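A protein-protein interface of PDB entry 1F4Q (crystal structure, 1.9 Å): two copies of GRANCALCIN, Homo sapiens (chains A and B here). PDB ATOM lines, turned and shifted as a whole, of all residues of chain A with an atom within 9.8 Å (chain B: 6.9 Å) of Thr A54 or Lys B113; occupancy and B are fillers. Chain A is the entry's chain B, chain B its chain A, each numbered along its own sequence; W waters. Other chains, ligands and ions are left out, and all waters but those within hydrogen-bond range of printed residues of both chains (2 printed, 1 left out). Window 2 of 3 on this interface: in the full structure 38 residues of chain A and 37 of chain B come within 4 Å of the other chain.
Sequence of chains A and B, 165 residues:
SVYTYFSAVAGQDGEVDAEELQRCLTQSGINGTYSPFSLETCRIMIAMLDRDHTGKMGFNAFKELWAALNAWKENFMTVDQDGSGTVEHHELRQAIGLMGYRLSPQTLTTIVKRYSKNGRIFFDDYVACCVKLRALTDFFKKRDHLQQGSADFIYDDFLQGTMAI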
ATOM      1  N   ASP A  13     -25.303  28.686 -16.750  1.00  0.00           N
ATOM      2  CA  ASP A  13     -23.943  28.199 -16.937  1.00  0.00           C
ATOM      3  C   ASP A  13     -23.391  28.761 -18.250  1.00  0.00           C
ATOM      4  O   ASP A  13     -22.264  28.454 -18.644  1.00  0.00           O
ATOM      5  CB  ASP A  13     -23.923  26.673 -16.978  1.00  0.00           C
ATOM      6  CG  ASP A  13     -24.942  26.106 -17.944  1.00  0.00           C
ATOM      7  OD1 ASP A  13     -25.461  26.872 -18.785  1.00  0.00           O
ATOM      8  OD2 ASP A  13     -25.220  24.890 -17.866  1.00  0.00           O
ATOM      9  N   GLU A  15     -24.514  28.109 -21.217  1.00  0.00           N
ATOM     10  CA  GLU A  15     -24.589  27.120 -22.284  1.00  0.00           C
ATOM     11  C   GLU A  15     -26.036  26.791 -22.627  1.00  0.00           C
ATOM     12  O   GLU A  15     -26.952  27.115 -21.872  1.00  0.00           O
ATOM     13  CB  GLU A  15     -23.877  25.838 -21.862  1.00  0.00           C
ATOM     14  CG  GLU A  15     -22.399  26.010 -21.556  1.00  0.00           C
ATOM     15  CD  GLU A  15     -21.745  24.697 -21.198  1.00  0.00           C
ATOM     16  OE1 GLU A  15     -22.088  24.130 -20.142  1.00  0.00           O
ATOM     17  OE2 GLU A  15     -20.894  24.227 -21.979  1.00  0.00           O
ATOM     18  N   VAL A  16     -26.232  26.145 -23.771  1.00  0.00           N
ATOM     19  CA  VAL A  16     -27.567  25.749 -24.192  1.00  0.00           C
ATOM     20  C   VAL A  16     -27.651  24.229 -24.290  1.00  0.00           C
ATOM     21  O   VAL A  16     -26.692  23.569 -24.708  1.00  0.00           O
ATOM     22  CB  VAL A  16     -27.934  26.337 -25.581  1.00  0.00           C
ATOM     23  CG1 VAL A  16     -27.980  27.856 -25.517  1.00  0.00           C
ATOM     24  CG2 VAL A  16     -26.930  25.883 -26.629  1.00  0.00           C
ATOM     25  N   ASP A  17     -28.778  23.673 -23.861  1.00  0.00           N
ATOM     26  CA  ASP A  17     -28.998  22.241 -23.992  1.00  0.00           C
ATOM     27  C   ASP A  17     -29.730  22.155 -25.338  1.00  0.00           C
ATOM     28  O   ASP A  17     -29.927  23.179 -25.987  1.00  0.00           O
ATOM     29  CB  ASP A  17     -29.846  21.692 -22.834  1.00  0.00           C
ATOM     30  CG  ASP A  17     -31.169  22.415 -22.664  1.00  0.00           C
ATOM     31  OD1 ASP A  17     -31.811  22.214 -21.612  1.00  0.00           O
ATOM     32  OD2 ASP A  17     -31.578  23.171 -23.566  1.00  0.00           O
ATOM     33  N   ALA A  18     -30.126  20.964 -25.766  1.00  0.00           N
ATOM     34  CA  ALA A  18     -30.788  20.824 -27.064  1.00  0.00           C
ATOM     35  C   ALA A  18     -32.058  21.657 -27.224  1.00  0.00           C
ATOM     36  O   ALA A  18     -32.283  22.252 -28.274  1.00  0.00           O
ATOM     37  CB  ALA A  18     -31.085  19.352 -27.341  1.00  0.00           C
ATOM     38  N   GLU A  19     -32.889  21.688 -26.191  1.00  0.00           N
ATOM     39  CA  GLU A  19     -34.135  22.449 -26.234  1.00  0.00           C
ATOM     40  C   GLU A  19     -33.846  23.939 -26.413  1.00  0.00           C
ATOM     41  O   GLU A  19     -34.495  24.618 -27.197  1.00  0.00           O
ATOM     42  CB  GLU A  19     -34.940  22.232 -24.945  1.00  0.00           C
ATOM     43  CG  GLU A  19     -35.568  20.845 -24.794  1.00  0.00           C
ATOM     44  CD  GLU A  19     -34.601  19.755 -24.332  1.00  0.00           C
ATOM     45  OE1 GLU A  19     -33.401  20.037 -24.104  1.00  0.00           O
ATOM     46  OE2 GLU A  19     -35.061  18.598 -24.190  1.00  0.00           O
ATOM     47  N   LEU A  39     -36.175  18.956 -32.503  1.00  0.00           N
ATOM     48  CA  LEU A  39     -35.377  18.707 -31.315  1.00  0.00           C
ATOM     49  C   LEU A  39     -34.316  17.647 -31.593  1.00  0.00           C
ATOM     50  O   LEU A  39     -33.175  17.780 -31.147  1.00  0.00           O
ATOM     51  CB  LEU A  39     -36.275  18.269 -30.151  1.00  0.00           C
ATOM     52  CG  LEU A  39     -35.590  17.984 -28.806  1.00  0.00           C
ATOM     53  CD1 LEU A  39     -34.953  19.262 -28.254  1.00  0.00           C
ATOM     54  CD2 LEU A  39     -36.615  17.439 -27.824  1.00  0.00           C
ATOM     55  N   CYS A  42     -31.364  19.127 -33.296  1.00  0.00           N
ATOM     56  CA  CYS A  42     -30.554  19.904 -32.357  1.00  0.00           C
ATOM     57  C   CYS A  42     -29.782  19.007 -31.392  1.00  0.00           C
ATOM     58  O   CYS A  42     -28.677  19.352 -30.951  1.00  0.00           O
ATOM     59  CB  CYS A  42     -31.437  20.896 -31.592  1.00  0.00           C
ATOM     60  SG  CYS A  42     -32.154  22.155 -32.678  1.00  0.00           S
ATOM     61  N   ARG A  43     -30.347  17.848 -31.065  1.00  0.00           N
ATOM     62  CA  ARG A  43     -29.652  16.922 -30.186  1.00  0.00           C
ATOM     63  C   ARG A  43     -28.414  16.387 -30.898  1.00  0.00           C
ATOM     64  O   ARG A  43     -27.368  16.182 -30.269  1.00  0.00           O
ATOM     65  CB  ARG A  43     -30.578  15.777 -29.771  1.00  0.00           C
ATOM     66  CG  ARG A  43     -31.419  16.130 -28.561  1.00  0.00           C
ATOM     67  CD  ARG A  43     -32.544  15.152 -28.307  1.00  0.00           C
ATOM     68  NE  ARG A  43     -33.254  15.491 -27.074  1.00  0.00           N
ATOM     69  CZ  ARG A  43     -34.389  14.920 -26.678  1.00  0.00           C
ATOM     70  NH1 ARG A  43     -34.963  13.982 -27.419  1.00  0.00           N
ATOM     71  NH2 ARG A  43     -34.938  15.276 -25.524  1.00  0.00           N
ATOM     72  N   ILE A  46     -25.695  19.041 -30.783  1.00  0.00           N
ATOM     73  CA  ILE A  46     -25.039  19.061 -29.480  1.00  0.00           C
ATOM     74  C   ILE A  46     -23.976  17.957 -29.443  1.00  0.00           C
ATOM     75  O   ILE A  46     -22.827  18.182 -29.040  1.00  0.00           O
ATOM     76  CB  ILE A  46     -26.061  18.805 -28.342  1.00  0.00           C
ATOM     77  CG1 ILE A  46     -27.030  19.993 -28.216  1.00  0.00           C
ATOM     78  CG2 ILE A  46     -25.330  18.537 -27.028  1.00  0.00           C
ATOM     79  CD1 ILE A  46     -26.405  21.271 -27.680  1.00  0.00           C
ATOM     80  N   ALA A  47     -24.368  16.758 -29.868  1.00  0.00           N
ATOM     81  CA  ALA A  47     -23.451  15.622 -29.869  1.00  0.00           C
ATOM     82  C   ALA A  47     -22.232  15.873 -30.744  1.00  0.00           C
ATOM     83  O   ALA A  47     -21.111  15.537 -30.367  1.00  0.00           O
ATOM     84  CB  ALA A  47     -24.178  14.365 -30.342  1.00  0.00           C
ATOM     85  N   LEU A  49     -20.553  18.481 -31.358  1.00  0.00           N
ATOM     86  CA  LEU A  49     -19.548  19.336 -30.726  1.00  0.00           C
ATOM     87  C   LEU A  49     -19.369  19.120 -29.226  1.00  0.00           C
ATOM     88  O   LEU A  49     -18.642  19.871 -28.570  1.00  0.00           O
ATOM     89  CB  LEU A  49     -19.898  20.808 -30.985  1.00  0.00           C
ATOM     90  CG  LEU A  49     -19.457  21.453 -32.308  1.00  0.00           C
ATOM     91  CD1 LEU A  49     -19.043  20.406 -33.319  1.00  0.00           C
ATOM     92  CD2 LEU A  49     -20.584  22.324 -32.838  1.00  0.00           C
ATOM     93  N   ASP A  50     -20.006  18.082 -28.692  1.00  0.00           N
ATOM     94  CA  ASP A  50     -19.940  17.785 -27.264  1.00  0.00           C
ATOM     95  C   ASP A  50     -18.610  17.156 -26.844  1.00  0.00           C
ATOM     96  O   ASP A  50     -18.567  15.988 -26.465  1.00  0.00           O
ATOM     97  CB  ASP A  50     -21.089  16.844 -26.886  1.00  0.00           C
ATOM     98  CG  ASP A  50     -21.348  16.805 -25.393  1.00  0.00           C
ATOM     99  OD1 ASP A  50     -20.562  17.407 -24.632  1.00  0.00           O
ATOM    100  OD2 ASP A  50     -22.340  16.168 -24.980  1.00  0.00           O
ATOM    101  N   ARG A  51     -17.531  17.930 -26.903  1.00  0.00           N
ATOM    102  CA  ARG A  51     -16.215  17.419 -26.523  1.00  0.00           C
ATOM    103  C   ARG A  51     -16.083  17.161 -25.022  1.00  0.00           C
ATOM    104  O   ARG A  51     -15.217  16.399 -24.593  1.00  0.00           O
ATOM    105  CB  ARG A  51     -15.108  18.380 -26.983  1.00  0.00           C
ATOM    106  CG  ARG A  51     -14.938  18.448 -28.497  1.00  0.00           C
ATOM    107  CD  ARG A  51     -13.679  19.206 -28.900  1.00  0.00           C
ATOM    108  NE  ARG A  51     -13.493  19.218 -30.352  1.00  0.00           N
ATOM    109  CZ  ARG A  51     -12.425  19.717 -30.969  1.00  0.00           C
ATOM    110  NH1 ARG A  51     -11.436  20.250 -30.264  1.00  0.00           N
ATOM    111  NH2 ARG A  51     -12.345  19.681 -32.292  1.00  0.00           N
ATOM    112  N   ASP A  52     -16.945  17.789 -24.226  1.00  0.00           N
ATOM    113  CA  ASP A  52     -16.904  17.608 -22.777  1.00  0.00           C
ATOM    114  C   ASP A  52     -17.865  16.532 -22.287  1.00  0.00           C
ATOM    115  O   ASP A  52     -17.874  16.202 -21.102  1.00  0.00           O
ATOM    116  CB  ASP A  52     -17.222  18.925 -22.060  1.00  0.00           C
ATOM    117  CG  ASP A  52     -16.087  19.925 -22.140  1.00  0.00           C
ATOM    118  OD1 ASP A  52     -16.230  21.032 -21.580  1.00  0.00           O
ATOM    119  OD2 ASP A  52     -15.050  19.607 -22.759  1.00  0.00           O
ATOM    120  N   HIS A  53     -18.672  15.988 -23.195  1.00  0.00           N
ATOM    121  CA  HIS A  53     -19.634  14.951 -22.829  1.00  0.00           C
ATOM    122  C   HIS A  53     -20.553  15.506 -21.741  1.00  0.00           C
ATOM    123  O   HIS A  53     -20.605  14.978 -20.627  1.00  0.00           O
ATOM    124  CB  HIS A  53     -18.896  13.719 -22.300  1.00  0.00           C
ATOM    125  CG  HIS A  53     -17.759  13.273 -23.168  1.00  0.00           C
ATOM    126  ND1 HIS A  53     -17.941  12.805 -24.452  1.00  0.00           N
ATOM    127  CD2 HIS A  53     -16.424  13.239 -22.941  1.00  0.00           C
ATOM    128  CE1 HIS A  53     -16.767  12.502 -24.978  1.00  0.00           C
ATOM    129  NE2 HIS A  53     -15.831  12.756 -24.082  1.00  0.00           N
ATOM    130  N   THR A  54     -21.283  16.567 -22.070  1.00  0.00           N
ATOM    131  CA  THR A  54     -22.169  17.211 -21.105  1.00  0.00           C
ATOM    132  C   THR A  54     -23.593  17.433 -21.608  1.00  0.00           C
ATOM    133  O   THR A  54     -24.478  17.795 -20.832  1.00  0.00           O
ATOM    134  CB  THR A  54     -21.610  18.581 -20.701  1.00  0.00           C
ATOM    135  OG1 THR A  54     -21.563  19.424 -21.861  1.00  0.00           O
ATOM    136  CG2 THR A  54     -20.201  18.441 -20.132  1.00  0.00           C
ATOM    137  N   GLY A  55     -23.813  17.229 -22.902  1.00  0.00           N
ATOM    138  CA  GLY A  55     -25.139  17.441 -23.455  1.00  0.00           C
ATOM    139  C   GLY A  55     -25.454  18.923 -23.588  1.00  0.00           C
ATOM    140  O   GLY A  55     -26.599  19.309 -23.835  1.00  0.00           O
ATOM    141  N   LYS A  56     -24.432  19.757 -23.425  1.00  0.00           N
ATOM    142  CA  LYS A  56     -24.601  21.201 -23.537  1.00  0.00           C
ATOM    143  C   LYS A  56     -23.575  21.812 -24.487  1.00  0.00           C
ATOM    144  O   LYS A  56     -22.599  21.160 -24.868  1.00  0.00           O
ATOM    145  CB  LYS A  56     -24.510  21.855 -22.159  1.00  0.00           C
ATOM    146  CG  LYS A  56     -25.685  21.510 -21.256  1.00  0.00           C
ATOM    147  CD  LYS A  56     -25.688  22.356 -19.999  1.00  0.00           C
ATOM    148  CE  LYS A  56     -26.955  22.133 -19.192  1.00  0.00           C
ATOM    149  NZ  LYS A  56     -26.987  22.994 -17.977  1.00  0.00           N
ATOM    150  N   MET A  57     -23.798  23.070 -24.857  1.00  0.00           N
ATOM    151  CA  MET A  57     -22.922  23.753 -25.799  1.00  0.00           C
ATOM    152  C   MET A  57     -22.667  25.207 -25.408  1.00  0.00           C
ATOM    153  O   MET A  57     -23.603  25.957 -25.167  1.00  0.00           O
ATOM    154  CB  MET A  57     -23.567  23.713 -27.191  1.00  0.00           C
ATOM    155  CG  MET A  57     -22.687  24.214 -28.320  1.00  0.00           C
ATOM    156  SD  MET A  57     -23.582  24.313 -29.899  1.00  0.00           S
ATOM    157  CE  MET A  57     -23.667  22.570 -30.361  1.00  0.00           C
ATOM    158  N   GLY A  58     -21.396  25.597 -25.356  1.00  0.00           N
ATOM    159  CA  GLY A  58     -21.053  26.970 -25.018  1.00  0.00           C
ATOM    160  C   GLY A  58     -21.077  27.801 -26.286  1.00  0.00           C
ATOM    161  O   GLY A  58     -21.275  27.261 -27.370  1.00  0.00           O
ATOM    162  N   ALA A  61     -18.401  26.926 -29.256  1.00  0.00           N
ATOM    163  CA  ALA A  61     -18.786  25.769 -30.055  1.00  0.00           C
ATOM    164  C   ALA A  61     -19.986  26.160 -30.918  1.00  0.00           C
ATOM    165  O   ALA A  61     -20.125  25.708 -32.057  1.00  0.00           O
ATOM    166  CB  ALA A  61     -19.144  24.603 -29.142  1.00  0.00           C
ATOM    167  N   GLN A 160     -22.012   3.944 -26.305  1.00  0.00           N
ATOM    168  CA  GLN A 160     -21.947   5.299 -25.773  1.00  0.00           C
ATOM    169  C   GLN A 160     -21.976   6.314 -26.904  1.00  0.00           C
ATOM    170  O   GLN A 160     -22.797   7.232 -26.905  1.00  0.00           O
ATOM    171  CB  GLN A 160     -20.670   5.517 -24.948  1.00  0.00           C
ATOM    172  CG  GLN A 160     -20.460   6.987 -24.568  1.00  0.00           C
ATOM    173  CD  GLN A 160     -19.270   7.215 -23.652  1.00  0.00           C
ATOM    174  OE1 GLN A 160     -18.124   6.953 -24.021  1.00  0.00           O
ATOM    175  NE2 GLN A 160     -19.540   7.711 -22.449  1.00  0.00           N
ATOM    176  N   MET A 163     -25.272   6.114 -29.164  1.00  0.00           N
ATOM    177  CA  MET A 163     -26.487   6.516 -28.450  1.00  0.00           C
ATOM    178  C   MET A 163     -26.460   8.039 -28.273  1.00  0.00           C
ATOM    179  O   MET A 163     -27.496   8.716 -28.320  1.00  0.00           O
ATOM    180  CB  MET A 163     -26.577   5.831 -27.083  1.00  0.00           C
ATOM    181  CG  MET A 163     -27.090   4.394 -27.123  1.00  0.00           C
ATOM    182  SD  MET A 163     -28.788   4.255 -27.748  1.00  0.00           S
ATOM    183  CE  MET A 163     -29.703   5.014 -26.406  1.00  0.00           C
ATOM    184  N   ALA A 164     -25.262   8.581 -28.091  1.00  0.00           N
ATOM    185  CA  ALA A 164     -25.106  10.017 -27.918  1.00  0.00           C
ATOM    186  C   ALA A 164     -25.492  10.785 -29.179  1.00  0.00           C
ATOM    187  O   ALA A 164     -26.159  11.818 -29.104  1.00  0.00           O
ATOM    188  CB  ALA A 164     -23.668  10.336 -27.541  1.00  0.00           C
ATOM    189  N   ILE A 165     -25.075  10.268 -30.333  1.00  0.00           N
ATOM    190  CA  ILE A 165     -25.337  10.906 -31.622  1.00  0.00           C
ATOM    191  C   ILE A 165     -26.740  10.622 -32.142  1.00  0.00           C
ATOM    192  O   ILE A 165     -27.475  11.598 -32.394  1.00  0.00           O
ATOM    193  CB  ILE A 165     -24.301  10.447 -32.677  1.00  0.00           C
ATOM    194  CG1 ILE A 165     -22.899  10.881 -32.239  1.00  0.00           C
ATOM    195  CG2 ILE A 165     -24.640  11.027 -34.058  1.00  0.00           C
ATOM    196  CD1 ILE A 165     -21.758  10.228 -33.035  1.00  0.00           C
ATOM    197  OXT ILE A 165     -27.085   9.434 -32.298  1.00  0.00           O
ATOM    198  N   HIS B  89     -33.492  11.013 -13.546  1.00  0.00           N
ATOM    199  CA  HIS B  89     -32.223  10.450 -14.010  1.00  0.00           C
ATOM    200  C   HIS B  89     -31.936   9.075 -13.414  1.00  0.00           C
ATOM    201  O   HIS B  89     -31.456   8.173 -14.105  1.00  0.00           O
ATOM    202  CB  HIS B  89     -31.058  11.388 -13.669  1.00  0.00           C
ATOM    203  CG  HIS B  89     -31.064  12.672 -14.438  1.00  0.00           C
ATOM    204  ND1 HIS B  89     -30.052  13.606 -14.329  1.00  0.00           N
ATOM    205  CD2 HIS B  89     -31.942  13.171 -15.336  1.00  0.00           C
ATOM    206  CE1 HIS B  89     -30.311  14.624 -15.131  1.00  0.00           C
ATOM    207  NE2 HIS B  89     -31.450  14.388 -15.754  1.00  0.00           N
ATOM    208  N   LEU B  92     -34.221   6.276 -15.110  1.00  0.00           N
ATOM    209  CA  LEU B  92     -33.920   5.904 -16.488  1.00  0.00           C
ATOM    210  C   LEU B  92     -32.771   4.901 -16.480  1.00  0.00           C
ATOM    211  O   LEU B  92     -32.828   3.876 -17.162  1.00  0.00           O
ATOM    212  CB  LEU B  92     -33.532   7.132 -17.317  1.00  0.00           C
ATOM    213  CG  LEU B  92     -33.197   6.831 -18.783  1.00  0.00           C
ATOM    214  CD1 LEU B  92     -34.390   6.174 -19.461  1.00  0.00           C
ATOM    215  CD2 LEU B  92     -32.815   8.112 -19.503  1.00  0.00           C
ATOM    216  N   LEU B 108     -24.016   5.290 -19.134  1.00  0.00           N
ATOM    217  CA  LEU B 108     -25.382   5.512 -18.666  1.00  0.00           C
ATOM    218  C   LEU B 108     -25.668   7.007 -18.524  1.00  0.00           C
ATOM    219  O   LEU B 108     -26.774   7.469 -18.812  1.00  0.00           O
ATOM    220  CB  LEU B 108     -25.603   4.810 -17.323  1.00  0.00           C
ATOM    221  CG  LEU B 108     -26.411   3.508 -17.344  1.00  0.00           C
ATOM    222  CD1 LEU B 108     -27.844   3.813 -17.721  1.00  0.00           C
ATOM    223  CD2 LEU B 108     -25.804   2.526 -18.322  1.00  0.00           C
ATOM    224  N   THR B 109     -24.665   7.754 -18.075  1.00  0.00           N
ATOM    225  CA  THR B 109     -24.794   9.197 -17.900  1.00  0.00           C
ATOM    226  C   THR B 109     -24.939   9.886 -19.254  1.00  0.00           C
ATOM    227  O   THR B 109     -25.756  10.792 -19.408  1.00  0.00           O
ATOM    228  CB  THR B 109     -23.559   9.780 -17.182  1.00  0.00           C
ATOM    229  OG1 THR B 109     -23.472   9.230 -15.863  1.00  0.00           O
ATOM    230  CG2 THR B 109     -23.654  11.294 -17.093  1.00  0.00           C
ATOM    231  N   THR B 110     -24.136   9.454 -20.223  1.00  0.00           N
ATOM    232  CA  THR B 110     -24.175  10.016 -21.569  1.00  0.00           C
ATOM    233  C   THR B 110     -25.555   9.806 -22.188  1.00  0.00           C
ATOM    234  O   THR B 110     -26.087  10.687 -22.870  1.00  0.00           O
ATOM    235  CB  THR B 110     -23.117   9.357 -22.481  1.00  0.00           C
ATOM    236  OG1 THR B 110     -21.812   9.561 -21.922  1.00  0.00           O
ATOM    237  CG2 THR B 110     -23.162   9.974 -23.879  1.00  0.00           C
ATOM    238  N   ILE B 111     -26.136   8.636 -21.951  1.00  0.00           N
ATOM    239  CA  ILE B 111     -27.461   8.339 -22.481  1.00  0.00           C
ATOM    240  C   ILE B 111     -28.496   9.243 -21.814  1.00  0.00           C
ATOM    241  O   ILE B 111     -29.327   9.855 -22.489  1.00  0.00           O
ATOM    242  CB  ILE B 111     -27.832   6.864 -22.243  1.00  0.00           C
ATOM    243  CG1 ILE B 111     -26.883   5.964 -23.032  1.00  0.00           C
ATOM    244  CG2 ILE B 111     -29.274   6.610 -22.665  1.00  0.00           C
ATOM    245  CD1 ILE B 111     -27.090   4.487 -22.781  1.00  0.00           C
ATOM    246  N   VAL B 112     -28.431   9.337 -20.487  1.00  0.00           N
ATOM    247  CA  VAL B 112     -29.353  10.169 -19.733  1.00  0.00           C
ATOM    248  C   VAL B 112     -29.229  11.651 -20.075  1.00  0.00           C
ATOM    249  O   VAL B 112     -30.232  12.362 -20.139  1.00  0.00           O
ATOM    250  CB  VAL B 112     -29.150   9.995 -18.208  1.00  0.00           C
ATOM    251  CG1 VAL B 112     -30.004  10.992 -17.442  1.00  0.00           C
ATOM    252  CG2 VAL B 112     -29.508   8.574 -17.796  1.00  0.00           C
ATOM    253  N   LYS B 113     -28.002  12.117 -20.299  1.00  0.00           N
ATOM    254  CA  LYS B 113     -27.766  13.519 -20.638  1.00  0.00           C
ATOM    255  C   LYS B 113     -28.274  13.930 -22.012  1.00  0.00           C
ATOM    256  O   LYS B 113     -28.507  15.119 -22.247  1.00  0.00           O
ATOM    257  CB  LYS B 113     -26.274  13.847 -20.534  1.00  0.00           C
ATOM    258  CG  LYS B 113     -25.822  14.102 -19.112  1.00  0.00           C
ATOM    259  CD  LYS B 113     -24.348  14.436 -19.041  1.00  0.00           C
ATOM    260  CE  LYS B 113     -24.002  15.056 -17.698  1.00  0.00           C
ATOM    261  NZ  LYS B 113     -24.416  14.214 -16.540  1.00  0.00           N
ATOM    262  N   ARG B 114     -28.447  12.973 -22.920  1.00  0.00           N
ATOM    263  CA  ARG B 114     -28.929  13.312 -24.261  1.00  0.00           C
ATOM    264  C   ARG B 114     -30.405  13.669 -24.249  1.00  0.00           C
ATOM    265  O   ARG B 114     -30.844  14.551 -24.989  1.00  0.00           O
ATOM    266  CB  ARG B 114     -28.726  12.163 -25.253  1.00  0.00           C
ATOM    267  CG  ARG B 114     -29.163  12.503 -26.694  1.00  0.00           C
ATOM    268  CD  ARG B 114     -28.980  11.313 -27.639  1.00  0.00           C
ATOM    269  NE  ARG B 114     -28.902  11.696 -29.051  1.00  0.00           N
ATOM    270  CZ  ARG B 114     -29.950  11.961 -29.827  1.00  0.00           C
ATOM    271  NH1 ARG B 114     -31.182  11.890 -29.341  1.00  0.00           N
ATOM    272  NH2 ARG B 114     -29.775  12.321 -31.090  1.00  0.00           N
ATOM    273  N   TYR B 115     -31.157  12.983 -23.404  1.00  0.00           N
ATOM    274  CA  TYR B 115     -32.604  13.183 -23.317  1.00  0.00           C
ATOM    275  C   TYR B 115     -33.084  14.039 -22.152  1.00  0.00           C
ATOM    276  O   TYR B 115     -34.162  14.623 -22.213  1.00  0.00           O
ATOM    277  CB  TYR B 115     -33.312  11.817 -23.249  1.00  0.00           C
ATOM    278  CG  TYR B 115     -33.059  10.915 -24.450  1.00  0.00           C
ATOM    279  CD1 TYR B 115     -33.586  11.224 -25.706  1.00  0.00           C
ATOM    280  CD2 TYR B 115     -32.267   9.766 -24.333  1.00  0.00           C
ATOM    281  CE1 TYR B 115     -33.329  10.419 -26.814  1.00  0.00           C
ATOM    282  CE2 TYR B 115     -32.000   8.959 -25.438  1.00  0.00           C
ATOM    283  CZ  TYR B 115     -32.533   9.296 -26.675  1.00  0.00           C
ATOM    284  OH  TYR B 115     -32.243   8.536 -27.782  1.00  0.00           O
ATOM    285  N   SER B 116     -32.286  14.106 -21.093  1.00  0.00           N
ATOM    286  CA  SER B 116     -32.643  14.870 -19.903  1.00  0.00           C
ATOM    287  C   SER B 116     -32.986  16.338 -20.137  1.00  0.00           C
ATOM    288  O   SER B 116     -32.274  17.054 -20.836  1.00  0.00           O
ATOM    289  CB  SER B 116     -31.518  14.795 -18.870  1.00  0.00           C
ATOM    290  OG  SER B 116     -31.778  15.674 -17.786  1.00  0.00           O
ATOM    291  N   LYS B 117     -34.086  16.779 -19.537  1.00  0.00           N
ATOM    292  CA  LYS B 117     -34.516  18.164 -19.636  1.00  0.00           C
ATOM    293  C   LYS B 117     -35.028  18.544 -18.257  1.00  0.00           C
ATOM    294  O   LYS B 117     -36.030  18.006 -17.788  1.00  0.00           O
ATOM    295  CB  LYS B 117     -35.621  18.326 -20.679  1.00  0.00           C
ATOM    296  CG  LYS B 117     -36.108  19.763 -20.833  1.00  0.00           C
ATOM    297  CD  LYS B 117     -34.953  20.730 -21.093  1.00  0.00           C
ATOM    298  CE  LYS B 117     -35.452  22.158 -21.276  1.00  0.00           C
ATOM    299  NZ  LYS B 117     -34.332  23.144 -21.315  1.00  0.00           N
HETATM  300  O   HOH W   1     -29.570  10.536 -33.962  1.00  0.00           O
HETATM  301  O   HOH W   2     -32.704  16.978 -24.643  1.00  0.00           O
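The side-chain hydroxyl (OG1) of Thr B110 is in hydrogen-bond range of the side-chain amide nitrogen (NE2) of Gln A160 (3.0 Å).
The backbone carbonyl oxygen (O) of Arg B114 is in hydrogen-bond range of the guanidinium group (NE) of Arg A43 (3.3 Å).
The guanidinium group (NE) of Arg B114 sits close to the backbone carbonyl oxygen (O) of Met A163, 3.4 Å away.
NE of Arg B114 sits at hydrogen-bond distance from O of Ala A164, at 2.7 Å.
The guanidinium group (NH2) of Arg B114 lies within salt-bridge range of the chain-end carboxylate (O) of Ile A165, at 2.7 Å.
The guanidinium group (NH2) of Arg A43 is in hydrogen-bond range of the backbone carbonyl oxygen (O) of Tyr B115, at 3.5 Å.
The side-chain amino group of Lys B117 is in salt-bridge range of the side-chain carboxylate of Asp A17, 2.7 Å away.
OD2 of Asp A17 lies within hydrogen-bond range of N of Glu A19 (3.3 Å).
NH2 of Arg A43 is in salt-bridge range of OE2 of Glu A19, 3.6 Å away.
The backbone NH (N) of Thr A54 sits at hydrogen-bond distance from the side-chain carboxylate (OD1) of Asp A50 (2.8 Å).
The side-chain hydroxyl of Thr A54 sits close to the backbone NH of Lys A56, 3.3 Å away.
Lys B117 touches Glu A19 (CD to CD, 3.4 Å).
O of Thr A54 touches CD of Lys B113, at 3.8 Å.
Thr B110 touches Ala A164 (CG2 to CB, 3.7 Å).
Of chain B, only Lys B113 (3.8 Å) comes within 4 Å of Thr A54.
Of the printed residues of chain A, Lys B113 touches Thr A54.
No residue of chain A comes within 4 Å of Val B112.
Of the printed residues of chain A, Lys B117 touches Asp A17 (2.7 Å) and Glu A19 (3.4 Å).
Of the printed residues of chain B, Ala A164 touches Thr B110 (3.7 Å) and Arg B114 (2.7 Å).
Of the printed residues of chain B, Gln A160 touches Thr B110 (3.0 Å).
Val A16 touches none of the printed residues of chain B.
The nearest residue of chain A that does not touch Lys B113 is His A53 (4.1 Å).
Hydrophobic or aromatic side chains of chain B within 4 Å of the printed part of chain A: Tyr B115.
Of the 26 printed residues of chain A, 8 touch a printed residue of chain B.
Printed residues of chain A that touch a printed residue of chain B: Asp A17, Glu A19, Arg A43, Thr A54, Gln A160, Met A163, Ala A164 and Ile A165.
Among the printed residues, 10 pairs touch across the chains.
No position is printed for both chains.
Of the 10 pairs that touch across the chains among the printed residues, none has its exchanged pair printed and touching as well.
Water W1 lies within hydrogen-bond range of O of Ile A165 (2.8 Å) and NH2 of Arg B114 (3.4 Å).
Water W2 lies within hydrogen-bond range of OE2 of Glu A19 (2.9 Å), NE of Arg A43 (2.9 Å) and O of Arg B114 (3.1 Å).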
